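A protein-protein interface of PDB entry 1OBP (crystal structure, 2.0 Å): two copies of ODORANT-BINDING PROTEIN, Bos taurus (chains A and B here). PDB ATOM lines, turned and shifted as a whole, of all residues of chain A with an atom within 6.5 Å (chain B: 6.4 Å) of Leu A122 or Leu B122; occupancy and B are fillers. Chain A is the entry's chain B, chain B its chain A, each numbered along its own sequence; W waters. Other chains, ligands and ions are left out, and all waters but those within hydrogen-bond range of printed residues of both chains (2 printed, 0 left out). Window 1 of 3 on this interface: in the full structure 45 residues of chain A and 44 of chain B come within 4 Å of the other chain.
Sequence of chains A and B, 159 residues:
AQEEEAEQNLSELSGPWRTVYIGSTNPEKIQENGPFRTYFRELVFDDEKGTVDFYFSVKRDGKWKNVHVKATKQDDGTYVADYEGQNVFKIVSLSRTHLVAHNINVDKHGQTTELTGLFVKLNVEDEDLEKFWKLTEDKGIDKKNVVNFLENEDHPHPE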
ATOM      1  N   GLY A  15     -18.445  27.584   6.442  1.00  0.00           N
ATOM      2  CA  GLY A  15     -19.599  27.217   5.647  1.00  0.00           C
ATOM      3  C   GLY A  15     -19.647  25.724   5.428  1.00  0.00           C
ATOM      4  O   GLY A  15     -18.963  24.988   6.137  1.00  0.00           O
ATOM      5  N   PRO A  16     -20.470  25.233   4.497  1.00  0.00           N
ATOM      6  CA  PRO A  16     -20.584  23.796   4.208  1.00  0.00           C
ATOM      7  C   PRO A  16     -19.334  23.255   3.503  1.00  0.00           C
ATOM      8  O   PRO A  16     -18.846  23.870   2.557  1.00  0.00           O
ATOM      9  CB  PRO A  16     -21.822  23.717   3.318  1.00  0.00           C
ATOM     10  CG  PRO A  16     -21.819  25.027   2.593  1.00  0.00           C
ATOM     11  CD  PRO A  16     -21.391  26.029   3.666  1.00  0.00           C
ATOM     12  N   TRP A  17     -18.833  22.119   3.975  1.00  0.00           N
ATOM     13  CA  TRP A  17     -17.627  21.470   3.429  1.00  0.00           C
ATOM     14  C   TRP A  17     -17.958  19.997   3.349  1.00  0.00           C
ATOM     15  O   TRP A  17     -18.832  19.507   4.087  1.00  0.00           O
ATOM     16  CB  TRP A  17     -16.408  21.686   4.353  1.00  0.00           C
ATOM     17  CG  TRP A  17     -15.723  23.081   4.290  1.00  0.00           C
ATOM     18  CD1 TRP A  17     -16.136  24.233   4.902  1.00  0.00           C
ATOM     19  CD2 TRP A  17     -14.498  23.421   3.594  1.00  0.00           C
ATOM     20  NE1 TRP A  17     -15.253  25.263   4.637  1.00  0.00           N
ATOM     21  CE2 TRP A  17     -14.241  24.794   3.839  1.00  0.00           C
ATOM     22  CE3 TRP A  17     -13.599  22.694   2.791  1.00  0.00           C
ATOM     23  CZ2 TRP A  17     -13.114  25.466   3.305  1.00  0.00           C
ATOM     24  CZ3 TRP A  17     -12.483  23.360   2.258  1.00  0.00           C
ATOM     25  CH2 TRP A  17     -12.250  24.736   2.520  1.00  0.00           C
ATOM     26  N   ARG A  18     -17.307  19.280   2.433  1.00  0.00           N
ATOM     27  CA  ARG A  18     -17.584  17.850   2.236  1.00  0.00           C
ATOM     28  C   ARG A  18     -16.283  17.043   2.141  1.00  0.00           C
ATOM     29  O   ARG A  18     -15.285  17.550   1.656  1.00  0.00           O
ATOM     30  CB  ARG A  18     -18.415  17.654   0.957  1.00  0.00           C
ATOM     31  CG  ARG A  18     -19.804  18.317   0.972  1.00  0.00           C
ATOM     32  CD  ARG A  18     -20.765  17.587   1.939  1.00  0.00           C
ATOM     33  NE  ARG A  18     -22.140  18.131   1.948  1.00  0.00           N
ATOM     34  CZ  ARG A  18     -22.576  19.136   2.718  1.00  0.00           C
ATOM     35  NH1 ARG A  18     -21.767  19.739   3.582  1.00  0.00           N
ATOM     36  NH2 ARG A  18     -23.845  19.539   2.629  1.00  0.00           N
ATOM     37  N   THR A  97     -11.513  27.019  -1.829  1.00  0.00           N
ATOM     38  CA  THR A  97     -12.235  25.825  -2.206  1.00  0.00           C
ATOM     39  C   THR A  97     -11.765  24.457  -1.710  1.00  0.00           C
ATOM     40  O   THR A  97     -12.545  23.511  -1.746  1.00  0.00           O
ATOM     41  CB  THR A  97     -12.458  25.779  -3.741  1.00  0.00           C
ATOM     42  OG1 THR A  97     -11.224  26.060  -4.427  1.00  0.00           O
ATOM     43  CG2 THR A  97     -13.515  26.822  -4.139  1.00  0.00           C
ATOM     44  N   VAL A 120     -13.634  19.588   0.341  1.00  0.00           N
ATOM     45  CA  VAL A 120     -13.928  20.676  -0.603  1.00  0.00           C
ATOM     46  C   VAL A 120     -15.079  21.521  -0.072  1.00  0.00           C
ATOM     47  O   VAL A 120     -15.962  20.997   0.616  1.00  0.00           O
ATOM     48  CB  VAL A 120     -14.332  20.129  -2.024  1.00  0.00           C
ATOM     49  CG1 VAL A 120     -15.575  19.235  -1.951  1.00  0.00           C
ATOM     50  CG2 VAL A 120     -14.598  21.282  -2.983  1.00  0.00           C
ATOM     51  N   LYS A 121     -15.077  22.813  -0.385  1.00  0.00           N
ATOM     52  CA  LYS A 121     -16.156  23.690   0.060  1.00  0.00           C
ATOM     53  C   LYS A 121     -17.289  23.818  -0.948  1.00  0.00           C
ATOM     54  O   LYS A 121     -17.026  23.882  -2.144  1.00  0.00           O
ATOM     55  CB  LYS A 121     -15.640  25.089   0.322  1.00  0.00           C
ATOM     56  CG  LYS A 121     -16.677  25.889   1.087  1.00  0.00           C
ATOM     57  CD  LYS A 121     -16.319  27.313   1.265  1.00  0.00           C
ATOM     58  CE  LYS A 121     -17.522  28.035   1.840  1.00  0.00           C
ATOM     59  NZ  LYS A 121     -17.174  29.435   2.062  1.00  0.00           N
ATOM     60  N   LEU A 122     -18.535  23.869  -0.467  1.00  0.00           N
ATOM     61  CA  LEU A 122     -19.706  24.063  -1.341  1.00  0.00           C
ATOM     62  C   LEU A 122     -19.941  25.563  -1.358  1.00  0.00           C
ATOM     63  O   LEU A 122     -20.372  26.143  -0.353  1.00  0.00           O
ATOM     64  CB  LEU A 122     -20.953  23.361  -0.799  1.00  0.00           C
ATOM     65  CG  LEU A 122     -21.330  22.051  -1.487  1.00  0.00           C
ATOM     66  CD1 LEU A 122     -20.137  21.093  -1.441  1.00  0.00           C
ATOM     67  CD2 LEU A 122     -22.559  21.417  -0.836  1.00  0.00           C
ATOM     68  N   ASN A 123     -19.659  26.184  -2.494  1.00  0.00           N
ATOM     69  CA  ASN A 123     -19.760  27.630  -2.663  1.00  0.00           C
ATOM     70  C   ASN A 123     -21.013  28.142  -3.335  1.00  0.00           C
ATOM     71  O   ASN A 123     -21.260  27.813  -4.493  1.00  0.00           O
ATOM     72  CB  ASN A 123     -18.569  28.121  -3.471  1.00  0.00           C
ATOM     73  CG  ASN A 123     -17.702  29.047  -2.695  1.00  0.00           C
ATOM     74  OD1 ASN A 123     -18.101  30.181  -2.415  1.00  0.00           O
ATOM     75  ND2 ASN A 123     -16.513  28.581  -2.310  1.00  0.00           N
ATOM     76  N   VAL A 124     -21.783  28.967  -2.631  1.00  0.00           N
ATOM     77  CA  VAL A 124     -23.002  29.540  -3.202  1.00  0.00           C
ATOM     78  C   VAL A 124     -22.829  31.044  -3.347  1.00  0.00           C
ATOM     79  O   VAL A 124     -22.738  31.765  -2.361  1.00  0.00           O
ATOM     80  CB  VAL A 124     -24.274  29.222  -2.357  1.00  0.00           C
ATOM     81  CG1 VAL A 124     -24.574  27.739  -2.382  1.00  0.00           C
ATOM     82  CG2 VAL A 124     -24.092  29.676  -0.918  1.00  0.00           C
ATOM     83  N   LEU A 150     -29.786  22.269   1.042  1.00  0.00           N
ATOM     84  CA  LEU A 150     -28.450  22.392   1.594  1.00  0.00           C
ATOM     85  C   LEU A 150     -28.408  22.310   3.134  1.00  0.00           C
ATOM     86  O   LEU A 150     -27.572  21.597   3.706  1.00  0.00           O
ATOM     87  CB  LEU A 150     -27.777  23.670   1.079  1.00  0.00           C
ATOM     88  CG  LEU A 150     -26.382  23.996   1.630  1.00  0.00           C
ATOM     89  CD1 LEU A 150     -25.398  22.845   1.396  1.00  0.00           C
ATOM     90  CD2 LEU A 150     -25.886  25.260   0.964  1.00  0.00           C
ATOM     91  N   GLU A 153     -29.075  18.685   4.497  1.00  0.00           N
ATOM     92  CA  GLU A 153     -27.881  17.855   4.440  1.00  0.00           C
ATOM     93  C   GLU A 153     -26.855  18.258   5.506  1.00  0.00           C
ATOM     94  O   GLU A 153     -26.137  17.405   5.985  1.00  0.00           O
ATOM     95  CB  GLU A 153     -27.235  17.916   3.063  1.00  0.00           C
ATOM     96  CG  GLU A 153     -27.847  16.962   2.043  1.00  0.00           C
ATOM     97  CD  GLU A 153     -27.052  16.914   0.739  1.00  0.00           C
ATOM     98  OE1 GLU A 153     -25.872  17.307   0.731  1.00  0.00           O
ATOM     99  OE2 GLU A 153     -27.603  16.497  -0.286  1.00  0.00           O
ATOM    100  N   ASP A 154     -26.770  19.549   5.845  1.00  0.00           N
ATOM    101  CA  ASP A 154     -25.826  20.046   6.861  1.00  0.00           C
ATOM    102  C   ASP A 154     -26.255  19.722   8.283  1.00  0.00           C
ATOM    103  O   ASP A 154     -25.492  19.950   9.229  1.00  0.00           O
ATOM    104  CB  ASP A 154     -25.649  21.571   6.767  1.00  0.00           C
ATOM    105  CG  ASP A 154     -24.727  22.007   5.623  1.00  0.00           C
ATOM    106  OD1 ASP A 154     -24.222  21.051   4.864  1.00  0.00           O
ATOM    107  OD2 ASP A 154     -24.467  23.202   5.445  1.00  0.00           O
ATOM    108  N   GLY B  15     -20.166  15.597 -13.350  1.00  0.00           N
ATOM    109  CA  GLY B  15     -19.517  15.393 -12.070  1.00  0.00           C
ATOM    110  C   GLY B  15     -20.529  15.439 -10.944  1.00  0.00           C
ATOM    111  O   GLY B  15     -21.719  15.309 -11.226  1.00  0.00           O
ATOM    112  N   PRO B  16     -20.086  15.477  -9.662  1.00  0.00           N
ATOM    113  CA  PRO B  16     -21.012  15.532  -8.522  1.00  0.00           C
ATOM    114  C   PRO B  16     -21.621  16.936  -8.384  1.00  0.00           C
ATOM    115  O   PRO B  16     -20.922  17.939  -8.501  1.00  0.00           O
ATOM    116  CB  PRO B  16     -20.116  15.149  -7.329  1.00  0.00           C
ATOM    117  CG  PRO B  16     -18.774  15.637  -7.725  1.00  0.00           C
ATOM    118  CD  PRO B  16     -18.695  15.288  -9.205  1.00  0.00           C
ATOM    119  N   TRP B  17     -22.940  16.995  -8.212  1.00  0.00           N
ATOM    120  CA  TRP B  17     -23.669  18.254  -8.058  1.00  0.00           C
ATOM    121  C   TRP B  17     -24.614  18.030  -6.888  1.00  0.00           C
ATOM    122  O   TRP B  17     -24.958  16.887  -6.572  1.00  0.00           O
ATOM    123  CB  TRP B  17     -24.528  18.568  -9.308  1.00  0.00           C
ATOM    124  CG  TRP B  17     -23.799  19.095 -10.516  1.00  0.00           C
ATOM    125  CD1 TRP B  17     -23.076  18.360 -11.417  1.00  0.00           C
ATOM    126  CD2 TRP B  17     -23.786  20.443 -10.994  1.00  0.00           C
ATOM    127  NE1 TRP B  17     -22.624  19.170 -12.430  1.00  0.00           N
ATOM    128  CE2 TRP B  17     -23.046  20.453 -12.198  1.00  0.00           C
ATOM    129  CE3 TRP B  17     -24.330  21.643 -10.530  1.00  0.00           C
ATOM    130  CZ2 TRP B  17     -22.835  21.626 -12.946  1.00  0.00           C
ATOM    131  CZ3 TRP B  17     -24.115  22.813 -11.273  1.00  0.00           C
ATOM    132  CH2 TRP B  17     -23.376  22.793 -12.465  1.00  0.00           C
ATOM    133  N   ARG B  18     -25.043  19.102  -6.246  1.00  0.00           N
ATOM    134  CA  ARG B  18     -25.953  18.967  -5.110  1.00  0.00           C
ATOM    135  C   ARG B  18     -27.103  19.970  -5.245  1.00  0.00           C
ATOM    136  O   ARG B  18     -26.943  21.041  -5.843  1.00  0.00           O
ATOM    137  CB  ARG B  18     -25.219  19.246  -3.763  1.00  0.00           C
ATOM    138  CG  ARG B  18     -24.085  18.271  -3.354  1.00  0.00           C
ATOM    139  CD  ARG B  18     -24.590  16.845  -3.119  1.00  0.00           C
ATOM    140  NE  ARG B  18     -23.515  15.888  -2.796  1.00  0.00           N
ATOM    141  CZ  ARG B  18     -22.894  15.100  -3.677  1.00  0.00           C
ATOM    142  NH1 ARG B  18     -23.211  15.136  -4.957  1.00  0.00           N
ATOM    143  NH2 ARG B  18     -21.986  14.228  -3.268  1.00  0.00           N
ATOM    144  N   THR B  97     -19.850  26.411 -11.844  1.00  0.00           N
ATOM    145  CA  THR B  97     -20.245  26.086 -10.486  1.00  0.00           C
ATOM    146  C   THR B  97     -21.736  25.993 -10.207  1.00  0.00           C
ATOM    147  O   THR B  97     -22.132  25.304  -9.269  1.00  0.00           O
ATOM    148  CB  THR B  97     -19.666  27.109  -9.479  1.00  0.00           C
ATOM    149  OG1 THR B  97     -20.097  28.432  -9.834  1.00  0.00           O
ATOM    150  CG2 THR B  97     -18.156  27.058  -9.474  1.00  0.00           C
ATOM    151  N   VAL B 120     -25.523  23.334  -7.196  1.00  0.00           N
ATOM    152  CA  VAL B 120     -24.126  23.788  -7.193  1.00  0.00           C
ATOM    153  C   VAL B 120     -23.196  22.605  -7.435  1.00  0.00           C
ATOM    154  O   VAL B 120     -23.509  21.476  -7.057  1.00  0.00           O
ATOM    155  CB  VAL B 120     -23.733  24.518  -5.873  1.00  0.00           C
ATOM    156  CG1 VAL B 120     -23.847  23.605  -4.694  1.00  0.00           C
ATOM    157  CG2 VAL B 120     -22.305  25.023  -5.960  1.00  0.00           C
ATOM    158  N   LYS B 121     -22.083  22.849  -8.113  1.00  0.00           N
ATOM    159  CA  LYS B 121     -21.152  21.772  -8.414  1.00  0.00           C
ATOM    160  C   LYS B 121     -20.063  21.611  -7.379  1.00  0.00           C
ATOM    161  O   LYS B 121     -19.602  22.585  -6.809  1.00  0.00           O
ATOM    162  CB  LYS B 121     -20.490  21.970  -9.779  1.00  0.00           C
ATOM    163  CG  LYS B 121     -19.755  20.711 -10.246  1.00  0.00           C
ATOM    164  CD  LYS B 121     -18.986  20.880 -11.540  1.00  0.00           C
ATOM    165  CE  LYS B 121     -18.372  19.540 -11.945  1.00  0.00           C
ATOM    166  NZ  LYS B 121     -17.545  19.668 -13.182  1.00  0.00           N
ATOM    167  N   LEU B 122     -19.676  20.373  -7.130  1.00  0.00           N
ATOM    168  CA  LEU B 122     -18.591  20.085  -6.199  1.00  0.00           C
ATOM    169  C   LEU B 122     -17.407  19.843  -7.111  1.00  0.00           C
ATOM    170  O   LEU B 122     -17.269  18.761  -7.657  1.00  0.00           O
ATOM    171  CB  LEU B 122     -18.874  18.814  -5.394  1.00  0.00           C
ATOM    172  CG  LEU B 122     -19.638  18.916  -4.074  1.00  0.00           C
ATOM    173  CD1 LEU B 122     -21.002  19.522  -4.304  1.00  0.00           C
ATOM    174  CD2 LEU B 122     -19.775  17.530  -3.462  1.00  0.00           C
ATOM    175  N   ASN B 123     -16.594  20.865  -7.321  1.00  0.00           N
ATOM    176  CA  ASN B 123     -15.457  20.728  -8.217  1.00  0.00           C
ATOM    177  C   ASN B 123     -14.158  20.348  -7.511  1.00  0.00           C
ATOM    178  O   ASN B 123     -13.743  20.993  -6.538  1.00  0.00           O
ATOM    179  CB  ASN B 123     -15.283  22.009  -9.045  1.00  0.00           C
ATOM    180  CG  ASN B 123     -14.244  21.861 -10.144  1.00  0.00           C
ATOM    181  OD1 ASN B 123     -13.355  22.717 -10.297  1.00  0.00           O
ATOM    182  ND2 ASN B 123     -14.329  20.764 -10.905  1.00  0.00           N
ATOM    183  N   VAL B 124     -13.555  19.254  -7.960  1.00  0.00           N
ATOM    184  CA  VAL B 124     -12.304  18.796  -7.374  1.00  0.00           C
ATOM    185  C   VAL B 124     -11.180  19.072  -8.377  1.00  0.00           C
ATOM    186  O   VAL B 124     -11.165  18.498  -9.465  1.00  0.00           O
ATOM    187  CB  VAL B 124     -12.362  17.296  -7.006  1.00  0.00           C
ATOM    188  CG1 VAL B 124     -11.023  16.853  -6.407  1.00  0.00           C
ATOM    189  CG2 VAL B 124     -13.498  17.054  -6.016  1.00  0.00           C
ATOM    190  N   LEU B 150     -17.126  10.625  -1.961  1.00  0.00           N
ATOM    191  CA  LEU B 150     -18.009  11.253  -2.930  1.00  0.00           C
ATOM    192  C   LEU B 150     -18.932  10.241  -3.615  1.00  0.00           C
ATOM    193  O   LEU B 150     -20.112  10.515  -3.840  1.00  0.00           O
ATOM    194  CB  LEU B 150     -17.181  12.065  -3.924  1.00  0.00           C
ATOM    195  CG  LEU B 150     -17.381  13.591  -3.974  1.00  0.00           C
ATOM    196  CD1 LEU B 150     -17.630  14.205  -2.606  1.00  0.00           C
ATOM    197  CD2 LEU B 150     -16.201  14.250  -4.645  1.00  0.00           C
HETATM  198  O   HOH W   1     -19.241  24.752  -4.782  1.00  0.00           O
HETATM  199  O   HOH W   2     -23.598  16.270   0.003  1.00  0.00           O
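The backbone carbonyl oxygen (O) of Pro B16 is in hydrogen-bond range of the backbone NH (N) of Leu B122 (3.1 Å).
N of Arg B18 sits at hydrogen-bond distance from O of Val B120 (2.9 Å).
N of Leu A122 lies within hydrogen-bond range of O of Pro A16, at 3.0 Å.
The backbone NH (N) of Arg A18 is in hydrogen-bond range of the backbone carbonyl oxygen (O) of Val A120 (2.8 Å).
Among the printed residues, merely in contact across the chains: Val A120 with Asn B123 (3.7 Å), Leu A122 with Leu B122 (3.4 Å) and Asn A123 with Val B120 (3.3 Å).
Leu A122 touches one residue of chain B.
Of the printed residues of chain A, Leu B122 touches Leu A122.
Printed residues of chain A within 4 Å of Asn B123: Val A120 (3.7 Å).
Of the printed residues of chain A, Val B120 touches Asn A123.
Printed residues of chain B within 4 Å of Val A120: Asn B123.
The nearest residue of chain A that does not touch Leu B122 is Arg A18 (4.5 Å).
Printed residues of chain A that touch a printed residue of chain B: Val A120, Leu A122 and Asn A123.
Hydrophobic or aromatic side chains of chain A within 4 Å of the printed part of chain B: Val A120 and Leu A122.
Among the printed residues, 3 pairs touch across the chains.
Among the printed residues, no Asp or Glu carboxylate lies within 4 Å of a Lys or Arg side-chain nitrogen of the other chain.
Val A120 touches Asn B123, and with the chains exchanged Asn A123 touches Val B120.
Leu B122 touches its own counterpart, Leu A122.
Positions printed for both chains: 15, 16, 17, 18, 97, 120, 121, 122, 123, 124 and 150.
Water W2 lies within hydrogen-bond range of the side-chain carboxylate of Glu A153 (2.6 Å), the guanidinium group of Arg B18 (2.8 Å) and the guanidinium group of Arg A18 (3.1 Å).
Water W1 lies within hydrogen-bond range of the backbone NH (N) of Asn A123 and the backbone carbonyl oxygen (O) of Lys B121.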
